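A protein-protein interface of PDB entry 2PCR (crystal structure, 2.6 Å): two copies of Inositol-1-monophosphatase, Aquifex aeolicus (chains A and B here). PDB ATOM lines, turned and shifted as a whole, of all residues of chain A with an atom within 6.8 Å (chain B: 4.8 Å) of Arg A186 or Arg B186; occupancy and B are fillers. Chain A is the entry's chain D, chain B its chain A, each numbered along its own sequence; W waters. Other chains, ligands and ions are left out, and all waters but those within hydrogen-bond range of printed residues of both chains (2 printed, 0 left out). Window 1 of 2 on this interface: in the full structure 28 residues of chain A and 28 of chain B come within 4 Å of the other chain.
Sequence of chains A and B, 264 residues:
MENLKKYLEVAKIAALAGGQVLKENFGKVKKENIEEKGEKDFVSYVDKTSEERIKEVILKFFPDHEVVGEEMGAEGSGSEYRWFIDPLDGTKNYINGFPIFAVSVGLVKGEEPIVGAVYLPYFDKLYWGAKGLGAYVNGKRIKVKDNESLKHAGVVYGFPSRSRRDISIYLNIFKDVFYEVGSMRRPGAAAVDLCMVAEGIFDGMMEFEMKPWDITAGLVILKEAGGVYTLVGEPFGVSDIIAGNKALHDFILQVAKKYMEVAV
The backbone carbonyl oxygen of Phe B159 lies within hydrogen-bond range of the guanidinium group of Arg B186, 2.7 Å away.
The backbone carbonyl oxygen of Asn A93 lies within hydrogen-bond range of the backbone NH of Phe A98 (2.9 Å).
The side-chain amide oxygen (OD1) of Asn A93 lies close to the backbone carbonyl oxygen (O) of Pro A187 (2.8 Å).
N of Arg A185 is in hydrogen-bond range of O of Val A155, at 2.8 Å.
The backbone carbonyl oxygen of Phe A159 lies within hydrogen-bond range of the guanidinium group of Arg A186 (3.2 Å).
N of Phe A178 is in hydrogen-bond range of SD of Met A184, 3.7 Å away.
Water W1 bridges NH2 of Arg A185 and O of Gly B188.
Water W2 lies within hydrogen-bond range of NH2 of Arg B185 (2.8 Å), O of Gly A188 (2.8 Å) and N of Asn A93 (3.1 Å).
CZ of Phe B178 touches O of Phe A159 (3.8 Å).
Phe B178 touches Pro A160 (CZ to O, 3.1 Å).
Phe B159 touches Phe A178.
Phe A178 touches Arg B186 (CE1 to NH2, 3.1 Å).
CA of Arg A185 touches O of Arg B186 (3.4 Å).
NE of Arg A185 touches CA of Gly B188, at 3.4 Å.
Arg A186 touches Phe B174 (NH1 to CZ, 3.2 Å).
Arg A186 touches Phe B178.
Arg A186 touches Arg B185.
Gly A188 touches Arg B185.
Tyr B157 touches its own counterpart, Tyr A157.
Tyr A157 touches Arg B186, and with the chains exchanged Arg A186 touches Tyr B157.
Phe A159 touches Phe B174, but with the chains exchanged Phe A174 does not touch Phe B159 (4.1 Å).
Phe A174 touches Arg B186, and with the chains exchanged Arg A186 touches Phe B174.
Of the 22 pairs that touch across the chains among the printed residues, 18 have their exchanged pair printed and touching as well.
The side-chain hydroxyl of Tyr B157 sits at hydrogen-bond distance from the side-chain hydroxyl of Tyr A157 (2.6 Å).
The side-chain hydroxyl (OH) of Tyr B157 lies close to the guanidinium group (NH1) of Arg A186 (3.4 Å).
The backbone carbonyl oxygen (O) of Phe B178 sits at hydrogen-bond distance from the side-chain hydroxyl (OG) of Ser A161 (3.2 Å).
The backbone carbonyl oxygen (O) of Met B184 lies close to the guanidinium group (NE) of Arg A186 (3.4 Å).
ND2 of Asn A93 sits close to NE of Arg B185 (2.8 Å).
O of Pro A187 sits close to NE of Arg B185 (3.3 Å).
The guanidinium group (NH1) of Arg B186 lies close to the side-chain hydroxyl (OH) of Tyr A157, 3.0 Å away.
NE of Arg B186 sits close to O of Met A184, 3.3 Å away.
N of Arg A186 sits at hydrogen-bond distance from O of Arg B186 (3.1 Å).
Printed residues of chain A that touch a printed residue of chain B: Asn A93, Tyr A157, Phe A159, Pro A160, Ser A161, Phe A174, Phe A178, Met A184, Arg A185, Arg A186, Pro A187 and Gly A188.
Of the 10 printed residues of chain B, 9 touch a printed residue of chain A.
Printed residues of chain B that touch a printed residue of chain A: Tyr B157, Phe B159, Phe B174, Phe B178, Met B184, Arg B185, Arg B186, Pro B187 and Gly B188.
Hydrophobic or aromatic side chains of chain B that line the printed part of chain A: Tyr B157, Phe B159, Phe B174, Phe B178 and Met B184.
Among the printed residues, no Asp or Glu carboxylate lies within 4 Å of a Lys or Arg side-chain nitrogen of the other chain.
Of the printed residues of chain B, Tyr A157 touches Tyr B157 (2.6 Å) and Arg B186 (2.9 Å).
Arg A186 touches just these residues of chain B: Tyr B157, Phe B174, Phe B178, Met B184, Arg B185 and Arg B186.
Asp A193 touches none of the printed residues of chain B.
Gly B158 touches none of the printed residues of chain A.
Of the printed residues of chain A, Phe B178 touches Phe A159, Pro A160, Ser A161 and Arg A186.
Of the printed residues of chain A, Arg B185 touches Asn A93 (2.8 Å), Arg A186 (3.2 Å), Pro A187 (3.1 Å) and Gly A188 (3.2 Å).
Printed residues of chain A within 4 Å of Arg B186: Tyr A157, Phe A174, Phe A178, Met A184, Arg A185 and Arg A186.
Of the printed residues of chain A, Pro B187 touches Arg A185.
The nearest printed residue of chain B that does not touch Arg A186 is Pro B187 (4.9 Å).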
ATOM      1  N   ASN A  93       5.130 -12.048  12.532  1.00  0.00           N
ATOM      2  CA  ASN A  93       4.251 -12.686  11.571  1.00  0.00           C
ATOM      3  C   ASN A  93       3.264 -11.632  11.071  1.00  0.00           C
ATOM      4  O   ASN A  93       2.999 -11.521   9.871  1.00  0.00           O
ATOM      5  CB  ASN A  93       3.494 -13.845  12.229  1.00  0.00           C
ATOM      6  CG  ASN A  93       4.361 -15.086  12.423  1.00  0.00           C
ATOM      7  OD1 ASN A  93       3.951 -16.043  13.085  1.00  0.00           O
ATOM      8  ND2 ASN A  93       5.554 -15.080  11.836  1.00  0.00           N
ATOM      9  N   PHE A  98       1.658 -12.898   7.700  1.00  0.00           N
ATOM     10  CA  PHE A  98       1.392 -14.316   7.967  1.00  0.00           C
ATOM     11  C   PHE A  98       0.342 -14.299   9.083  1.00  0.00           C
ATOM     12  O   PHE A  98       0.616 -13.863  10.203  1.00  0.00           O
ATOM     13  CB  PHE A  98       2.686 -15.013   8.404  1.00  0.00           C
ATOM     14  CG  PHE A  98       2.547 -16.495   8.590  1.00  0.00           C
ATOM     15  CD1 PHE A  98       2.020 -17.293   7.578  1.00  0.00           C
ATOM     16  CD2 PHE A  98       2.950 -17.101   9.779  1.00  0.00           C
ATOM     17  CE1 PHE A  98       1.896 -18.668   7.745  1.00  0.00           C
ATOM     18  CE2 PHE A  98       2.831 -18.481   9.953  1.00  0.00           C
ATOM     19  CZ  PHE A  98       2.301 -19.267   8.932  1.00  0.00           C
ATOM     20  N   VAL A 155       4.421 -31.636  17.042  1.00  0.00           N
ATOM     21  CA  VAL A 155       4.881 -30.684  18.038  1.00  0.00           C
ATOM     22  C   VAL A 155       5.255 -29.317  17.467  1.00  0.00           C
ATOM     23  O   VAL A 155       5.900 -29.220  16.425  1.00  0.00           O
ATOM     24  CB  VAL A 155       6.106 -31.275  18.800  1.00  0.00           C
ATOM     25  CG1 VAL A 155       6.799 -30.208  19.629  1.00  0.00           C
ATOM     26  CG2 VAL A 155       5.644 -32.412  19.693  1.00  0.00           C
ATOM     27  N   VAL A 156       4.828 -28.257  18.144  1.00  0.00           N
ATOM     28  CA  VAL A 156       5.196 -26.914  17.713  1.00  0.00           C
ATOM     29  C   VAL A 156       6.344 -26.488  18.634  1.00  0.00           C
ATOM     30  O   VAL A 156       6.337 -26.805  19.820  1.00  0.00           O
ATOM     31  CB  VAL A 156       4.025 -25.902  17.849  1.00  0.00           C
ATOM     32  CG1 VAL A 156       2.931 -26.230  16.848  1.00  0.00           C
ATOM     33  CG2 VAL A 156       3.472 -25.924  19.261  1.00  0.00           C
ATOM     34  N   TYR A 157       7.344 -25.805  18.086  1.00  0.00           N
ATOM     35  CA  TYR A 157       8.473 -25.346  18.895  1.00  0.00           C
ATOM     36  C   TYR A 157       8.805 -23.881  18.634  1.00  0.00           C
ATOM     37  O   TYR A 157       8.160 -23.216  17.821  1.00  0.00           O
ATOM     38  CB  TYR A 157       9.725 -26.191  18.631  1.00  0.00           C
ATOM     39  CG  TYR A 157      10.221 -26.155  17.205  1.00  0.00           C
ATOM     40  CD1 TYR A 157       9.592 -26.904  16.210  1.00  0.00           C
ATOM     41  CD2 TYR A 157      11.339 -25.398  16.853  1.00  0.00           C
ATOM     42  CE1 TYR A 157      10.070 -26.912  14.902  1.00  0.00           C
ATOM     43  CE2 TYR A 157      11.824 -25.397  15.543  1.00  0.00           C
ATOM     44  CZ  TYR A 157      11.187 -26.161  14.574  1.00  0.00           C
ATOM     45  OH  TYR A 157      11.689 -26.203  13.291  1.00  0.00           O
ATOM     46  N   GLY A 158       9.817 -23.391  19.337  1.00  0.00           N
ATOM     47  CA  GLY A 158      10.232 -22.018  19.165  1.00  0.00           C
ATOM     48  C   GLY A 158      11.203 -21.561  20.226  1.00  0.00           C
ATOM     49  O   GLY A 158      11.138 -21.990  21.380  1.00  0.00           O
ATOM     50  N   PHE A 159      12.130 -20.705  19.819  1.00  0.00           N
ATOM     51  CA  PHE A 159      13.113 -20.134  20.730  1.00  0.00           C
ATOM     52  C   PHE A 159      13.564 -18.787  20.193  1.00  0.00           C
ATOM     53  O   PHE A 159      13.396 -18.494  19.010  1.00  0.00           O
ATOM     54  CB  PHE A 159      14.314 -21.072  20.948  1.00  0.00           C
ATOM     55  CG  PHE A 159      14.757 -21.814  19.721  1.00  0.00           C
ATOM     56  CD1 PHE A 159      14.080 -22.952  19.298  1.00  0.00           C
ATOM     57  CD2 PHE A 159      15.878 -21.403  19.013  1.00  0.00           C
ATOM     58  CE1 PHE A 159      14.519 -23.672  18.188  1.00  0.00           C
ATOM     59  CE2 PHE A 159      16.323 -22.114  17.904  1.00  0.00           C
ATOM     60  CZ  PHE A 159      15.643 -23.252  17.491  1.00  0.00           C
ATOM     61  N   PRO A 160      14.134 -17.942  21.063  1.00  0.00           N
ATOM     62  CA  PRO A 160      14.602 -16.613  20.666  1.00  0.00           C
ATOM     63  C   PRO A 160      15.909 -16.600  19.890  1.00  0.00           C
ATOM     64  O   PRO A 160      16.682 -17.560  19.920  1.00  0.00           O
ATOM     65  CB  PRO A 160      14.736 -15.895  21.999  1.00  0.00           C
ATOM     66  CG  PRO A 160      15.246 -16.984  22.881  1.00  0.00           C
ATOM     67  CD  PRO A 160      14.347 -18.154  22.507  1.00  0.00           C
ATOM     68  N   SER A 161      16.145 -15.491  19.196  1.00  0.00           N
ATOM     69  CA  SER A 161      17.367 -15.301  18.424  1.00  0.00           C
ATOM     70  C   SER A 161      18.291 -14.436  19.288  1.00  0.00           C
ATOM     71  O   SER A 161      17.797 -13.437  19.849  1.00  0.00           O
ATOM     72  CB  SER A 161      17.055 -14.596  17.093  1.00  0.00           C
ATOM     73  OG  SER A 161      18.201 -14.512  16.264  1.00  0.00           O
ATOM     74  N   PHE A 174      15.625 -29.951  20.497  1.00  0.00           N
ATOM     75  CA  PHE A 174      14.837 -30.014  19.266  1.00  0.00           C
ATOM     76  C   PHE A 174      15.170 -31.286  18.496  1.00  0.00           C
ATOM     77  O   PHE A 174      14.283 -32.028  18.077  1.00  0.00           O
ATOM     78  CB  PHE A 174      15.141 -28.805  18.368  1.00  0.00           C
ATOM     79  CG  PHE A 174      14.692 -28.987  16.942  1.00  0.00           C
ATOM     80  CD1 PHE A 174      13.350 -28.848  16.594  1.00  0.00           C
ATOM     81  CD2 PHE A 174      15.601 -29.366  15.956  1.00  0.00           C
ATOM     82  CE1 PHE A 174      12.917 -29.091  15.279  1.00  0.00           C
ATOM     83  CE2 PHE A 174      15.180 -29.612  14.642  1.00  0.00           C
ATOM     84  CZ  PHE A 174      13.836 -29.475  14.305  1.00  0.00           C
ATOM     85  N   PHE A 178      12.720 -34.172  17.579  1.00  0.00           N
ATOM     86  CA  PHE A 178      12.561 -34.234  16.132  1.00  0.00           C
ATOM     87  C   PHE A 178      12.656 -35.670  15.646  1.00  0.00           C
ATOM     88  O   PHE A 178      11.829 -36.127  14.864  1.00  0.00           O
ATOM     89  CB  PHE A 178      13.653 -33.378  15.469  1.00  0.00           C
ATOM     90  CG  PHE A 178      13.515 -33.227  13.977  1.00  0.00           C
ATOM     91  CD1 PHE A 178      12.367 -32.675  13.418  1.00  0.00           C
ATOM     92  CD2 PHE A 178      14.570 -33.572  13.133  1.00  0.00           C
ATOM     93  CE1 PHE A 178      12.273 -32.462  12.037  1.00  0.00           C
ATOM     94  CE2 PHE A 178      14.487 -33.362  11.756  1.00  0.00           C
ATOM     95  CZ  PHE A 178      13.335 -32.805  11.206  1.00  0.00           C
ATOM     96  N   SER A 183       5.932 -34.979  13.314  1.00  0.00           N
ATOM     97  CA  SER A 183       6.167 -33.660  12.754  1.00  0.00           C
ATOM     98  C   SER A 183       6.424 -32.583  13.788  1.00  0.00           C
ATOM     99  O   SER A 183       5.999 -32.678  14.942  1.00  0.00           O
ATOM    100  CB  SER A 183       4.974 -33.239  11.907  1.00  0.00           C
ATOM    101  OG  SER A 183       3.802 -33.221  12.697  1.00  0.00           O
ATOM    102  N   MET A 184       7.126 -31.547  13.350  1.00  0.00           N
ATOM    103  CA  MET A 184       7.406 -30.407  14.191  1.00  0.00           C
ATOM    104  C   MET A 184       7.253 -29.134  13.385  1.00  0.00           C
ATOM    105  O   MET A 184       7.813 -28.993  12.305  1.00  0.00           O
ATOM    106  CB  MET A 184       8.797 -30.521  14.799  1.00  0.00           C
ATOM    107  CG  MET A 184       8.746 -31.222  16.140  1.00  0.00           C
ATOM    108  SD  MET A 184      10.430 -31.284  17.030  1.00  0.00           S
ATOM    109  CE  MET A 184      10.276 -29.699  18.123  1.00  0.00           C
ATOM    110  N   ARG A 185       6.458 -28.219  13.919  1.00  0.00           N
ATOM    111  CA  ARG A 185       6.181 -26.957  13.259  1.00  0.00           C
ATOM    112  C   ARG A 185       6.621 -25.781  14.113  1.00  0.00           C
ATOM    113  O   ARG A 185       6.820 -25.906  15.323  1.00  0.00           O
ATOM    114  CB  ARG A 185       4.681 -26.858  12.966  1.00  0.00           C
ATOM    115  CG  ARG A 185       4.133 -28.045  12.180  1.00  0.00           C
ATOM    116  CD  ARG A 185       4.528 -27.954  10.726  1.00  0.00           C
ATOM    117  NE  ARG A 185       4.251 -29.175   9.973  1.00  0.00           N
ATOM    118  CZ  ARG A 185       5.173 -30.078   9.648  1.00  0.00           C
ATOM    119  NH1 ARG A 185       6.434 -29.909  10.011  1.00  0.00           N
ATOM    120  NH2 ARG A 185       4.832 -31.148   8.943  1.00  0.00           N
ATOM    121  N   ARG A 186       6.764 -24.632  13.471  1.00  0.00           N
ATOM    122  CA  ARG A 186       7.172 -23.421  14.154  1.00  0.00           C
ATOM    123  C   ARG A 186       6.318 -22.263  13.646  1.00  0.00           C
ATOM    124  O   ARG A 186       6.767 -21.452  12.844  1.00  0.00           O
ATOM    125  CB  ARG A 186       8.645 -23.154  13.865  1.00  0.00           C
ATOM    126  CG  ARG A 186       9.237 -22.040  14.694  1.00  0.00           C
ATOM    127  CD  ARG A 186      10.665 -21.799  14.299  1.00  0.00           C
ATOM    128  NE  ARG A 186      11.325 -20.915  15.244  1.00  0.00           N
ATOM    129  CZ  ARG A 186      12.565 -20.473  15.100  1.00  0.00           C
ATOM    130  NH1 ARG A 186      13.277 -20.837  14.041  1.00  0.00           N
ATOM    131  NH2 ARG A 186      13.091 -19.671  16.014  1.00  0.00           N
ATOM    132  N   PRO A 187       5.064 -22.185  14.103  1.00  0.00           N
ATOM    133  CA  PRO A 187       4.145 -21.120  13.681  1.00  0.00           C
ATOM    134  C   PRO A 187       4.583 -19.688  14.007  1.00  0.00           C
ATOM    135  O   PRO A 187       4.305 -18.774  13.235  1.00  0.00           O
ATOM    136  CB  PRO A 187       2.840 -21.507  14.362  1.00  0.00           C
ATOM    137  CG  PRO A 187       2.933 -23.027  14.389  1.00  0.00           C
ATOM    138  CD  PRO A 187       4.348 -23.219  14.868  1.00  0.00           C
ATOM    139  N   GLY A 188       5.238 -19.495  15.152  1.00  0.00           N
ATOM    140  CA  GLY A 188       5.716 -18.169  15.525  1.00  0.00           C
ATOM    141  C   GLY A 188       4.885 -17.332  16.481  1.00  0.00           C
ATOM    142  O   GLY A 188       5.047 -16.114  16.534  1.00  0.00           O
ATOM    143  N   ALA A 189       3.994 -17.971  17.232  1.00  0.00           N
ATOM    144  CA  ALA A 189       3.154 -17.263  18.201  1.00  0.00           C
ATOM    145  C   ALA A 189       2.726 -18.214  19.323  1.00  0.00           C
ATOM    146  O   ALA A 189       1.766 -18.981  19.185  1.00  0.00           O
ATOM    147  CB  ALA A 189       1.936 -16.674  17.504  1.00  0.00           C
ATOM    148  N   ASP A 193       0.018 -21.105  19.795  1.00  0.00           N
ATOM    149  CA  ASP A 193       0.532 -22.467  19.946  1.00  0.00           C
ATOM    150  C   ASP A 193      -0.248 -23.210  21.042  1.00  0.00           C
ATOM    151  O   ASP A 193      -0.839 -24.261  20.802  1.00  0.00           O
ATOM    152  CB  ASP A 193       2.017 -22.442  20.336  1.00  0.00           C
ATOM    153  CG  ASP A 193       2.941 -22.114  19.172  1.00  0.00           C
ATOM    154  OD1 ASP A 193       4.160 -21.964  19.415  1.00  0.00           O
ATOM    155  OD2 ASP A 193       2.462 -22.013  18.024  1.00  0.00           O
ATOM    156  N   GLU A 207       8.603 -24.199  24.122  1.00  0.00           N
ATOM    157  CA  GLU A 207       8.938 -22.819  23.804  1.00  0.00           C
ATOM    158  C   GLU A 207       9.892 -22.282  24.880  1.00  0.00           C
ATOM    159  O   GLU A 207       9.667 -22.465  26.080  1.00  0.00           O
ATOM    160  CB  GLU A 207       7.657 -21.995  23.769  1.00  0.00           C
ATOM    161  CG  GLU A 207       7.783 -20.651  23.101  1.00  0.00           C
ATOM    162  CD  GLU A 207       7.263 -20.653  21.684  1.00  0.00           C
ATOM    163  OE1 GLU A 207       6.392 -21.496  21.363  1.00  0.00           O
ATOM    164  OE2 GLU A 207       7.718 -19.797  20.896  1.00  0.00           O
ATOM    165  N   TYR B 157      11.502 -22.537   6.421  1.00  0.00           N
ATOM    166  CA  TYR B 157      12.436 -23.628   6.148  1.00  0.00           C
ATOM    167  C   TYR B 157      11.818 -24.999   6.375  1.00  0.00           C
ATOM    168  O   TYR B 157      10.678 -25.124   6.830  1.00  0.00           O
ATOM    169  CB  TYR B 157      13.675 -23.487   7.039  1.00  0.00           C
ATOM    170  CG  TYR B 157      13.377 -23.586   8.520  1.00  0.00           C
ATOM    171  CD1 TYR B 157      13.501 -24.802   9.201  1.00  0.00           C
ATOM    172  CD2 TYR B 157      12.967 -22.461   9.246  1.00  0.00           C
ATOM    173  CE1 TYR B 157      13.230 -24.892  10.579  1.00  0.00           C
ATOM    174  CE2 TYR B 157      12.692 -22.540  10.616  1.00  0.00           C
ATOM    175  CZ  TYR B 157      12.830 -23.756  11.276  1.00  0.00           C
ATOM    176  OH  TYR B 157      12.607 -23.819  12.634  1.00  0.00           O
ATOM    177  N   GLY B 158      12.593 -26.028   6.053  1.00  0.00           N
ATOM    178  CA  GLY B 158      12.120 -27.380   6.236  1.00  0.00           C
ATOM    179  C   GLY B 158      13.106 -28.445   5.814  1.00  0.00           C
ATOM    180  O   GLY B 158      13.791 -28.306   4.805  1.00  0.00           O
ATOM    181  N   PHE B 159      13.181 -29.501   6.617  1.00  0.00           N
ATOM    182  CA  PHE B 159      14.033 -30.662   6.354  1.00  0.00           C
ATOM    183  C   PHE B 159      13.409 -31.882   7.041  1.00  0.00           C
ATOM    184  O   PHE B 159      12.686 -31.748   8.027  1.00  0.00           O
ATOM    185  CB  PHE B 159      15.486 -30.440   6.834  1.00  0.00           C
ATOM    186  CG  PHE B 159      15.611 -29.807   8.190  1.00  0.00           C
ATOM    187  CD1 PHE B 159      15.864 -28.443   8.309  1.00  0.00           C
ATOM    188  CD2 PHE B 159      15.522 -30.575   9.347  1.00  0.00           C
ATOM    189  CE1 PHE B 159      16.035 -27.851   9.563  1.00  0.00           C
ATOM    190  CE2 PHE B 159      15.690 -29.989  10.611  1.00  0.00           C
ATOM    191  CZ  PHE B 159      15.949 -28.626  10.715  1.00  0.00           C
ATOM    192  N   PHE B 174      20.725 -23.784   9.681  1.00  0.00           N
ATOM    193  CA  PHE B 174      19.673 -23.137  10.465  1.00  0.00           C
ATOM    194  C   PHE B 174      20.210 -22.035  11.375  1.00  0.00           C
ATOM    195  O   PHE B 174      19.689 -20.921  11.373  1.00  0.00           O
ATOM    196  CB  PHE B 174      18.930 -24.197  11.293  1.00  0.00           C
ATOM    197  CG  PHE B 174      17.900 -23.638  12.231  1.00  0.00           C
ATOM    198  CD1 PHE B 174      18.268 -23.152  13.482  1.00  0.00           C
ATOM    199  CD2 PHE B 174      16.553 -23.597  11.864  1.00  0.00           C
ATOM    200  CE1 PHE B 174      17.312 -22.633  14.358  1.00  0.00           C
ATOM    201  CE2 PHE B 174      15.591 -23.080  12.734  1.00  0.00           C
ATOM    202  CZ  PHE B 174      15.972 -22.597  13.982  1.00  0.00           C
ATOM    203  N   PHE B 178      19.594 -18.273  11.175  1.00  0.00           N
ATOM    204  CA  PHE B 178      18.835 -17.865  12.357  1.00  0.00           C
ATOM    205  C   PHE B 178      19.354 -16.567  12.990  1.00  0.00           C
ATOM    206  O   PHE B 178      18.580 -15.663  13.306  1.00  0.00           O
ATOM    207  CB  PHE B 178      18.853 -19.002  13.393  1.00  0.00           C
ATOM    208  CG  PHE B 178      18.027 -18.730  14.616  1.00  0.00           C
ATOM    209  CD1 PHE B 178      16.639 -18.692  14.541  1.00  0.00           C
ATOM    210  CD2 PHE B 178      18.641 -18.483  15.840  1.00  0.00           C
ATOM    211  CE1 PHE B 178      15.871 -18.411  15.666  1.00  0.00           C
ATOM    212  CE2 PHE B 178      17.884 -18.201  16.969  1.00  0.00           C
ATOM    213  CZ  PHE B 178      16.492 -18.164  16.883  1.00  0.00           C
ATOM    214  N   MET B 184      12.189 -16.919  11.482  1.00  0.00           N
ATOM    215  CA  MET B 184      12.188 -18.176  10.753  1.00  0.00           C
ATOM    216  C   MET B 184      10.982 -19.009  11.143  1.00  0.00           C
ATOM    217  O   MET B 184      10.710 -19.220  12.326  1.00  0.00           O
ATOM    218  CB  MET B 184      13.448 -18.971  11.041  1.00  0.00           C
ATOM    219  CG  MET B 184      14.678 -18.376  10.435  1.00  0.00           C
ATOM    220  SD  MET B 184      16.090 -19.632  10.596  1.00  0.00           S
ATOM    221  CE  MET B 184      15.969 -20.463   8.855  1.00  0.00           C
ATOM    222  N   ARG B 185      10.264 -19.484  10.133  1.00  0.00           N
ATOM    223  CA  ARG B 185       9.071 -20.278  10.355  1.00  0.00           C
ATOM    224  C   ARG B 185       9.105 -21.613   9.611  1.00  0.00           C
ATOM    225  O   ARG B 185       9.648 -21.723   8.512  1.00  0.00           O
ATOM    226  CB  ARG B 185       7.851 -19.461   9.936  1.00  0.00           C
ATOM    227  CG  ARG B 185       7.712 -18.154  10.703  1.00  0.00           C
ATOM    228  CD  ARG B 185       7.137 -18.371  12.095  1.00  0.00           C
ATOM    229  NE  ARG B 185       7.117 -17.142  12.885  1.00  0.00           N
ATOM    230  CZ  ARG B 185       8.109 -16.732  13.677  1.00  0.00           C
ATOM    231  NH1 ARG B 185       9.219 -17.453  13.802  1.00  0.00           N
ATOM    232  NH2 ARG B 185       7.996 -15.592  14.347  1.00  0.00           N
ATOM    233  N   ARG B 186       8.517 -22.628  10.234  1.00  0.00           N
ATOM    234  CA  ARG B 186       8.457 -23.966   9.667  1.00  0.00           C
ATOM    235  C   ARG B 186       6.985 -24.381   9.582  1.00  0.00           C
ATOM    236  O   ARG B 186       6.498 -25.171  10.391  1.00  0.00           O
ATOM    237  CB  ARG B 186       9.233 -24.920  10.567  1.00  0.00           C
ATOM    238  CG  ARG B 186       9.235 -26.346  10.102  1.00  0.00           C
ATOM    239  CD  ARG B 186      10.049 -27.183  11.044  1.00  0.00           C
ATOM    240  NE  ARG B 186      10.492 -28.410  10.406  1.00  0.00           N
ATOM    241  CZ  ARG B 186      11.665 -28.981  10.646  1.00  0.00           C
ATOM    242  NH1 ARG B 186      12.502 -28.427  11.514  1.00  0.00           N
ATOM    243  NH2 ARG B 186      12.003 -30.095  10.013  1.00  0.00           N
ATOM    244  N   PRO B 187       6.255 -23.837   8.597  1.00  0.00           N
ATOM    245  CA  PRO B 187       4.832 -24.119   8.379  1.00  0.00           C
ATOM    246  C   PRO B 187       4.458 -25.562   8.059  1.00  0.00           C
ATOM    247  O   PRO B 187       3.396 -26.023   8.466  1.00  0.00           O
ATOM    248  CB  PRO B 187       4.468 -23.153   7.258  1.00  0.00           C
ATOM    249  CG  PRO B 187       5.395 -22.000   7.516  1.00  0.00           C
ATOM    250  CD  PRO B 187       6.690 -22.732   7.733  1.00  0.00           C
ATOM    251  N   GLY B 188       5.311 -26.260   7.313  1.00  0.00           N
ATOM    252  CA  GLY B 188       5.038 -27.654   6.990  1.00  0.00           C
ATOM    253  C   GLY B 188       4.524 -28.046   5.607  1.00  0.00           C
ATOM    254  O   GLY B 188       4.052 -29.172   5.423  1.00  0.00           O
HETATM  255  O   HOH W   1       2.811 -31.241   7.081  1.00  0.00           O
HETATM  256  O   HOH W   2       5.828 -13.908  14.950  1.00  0.00           O
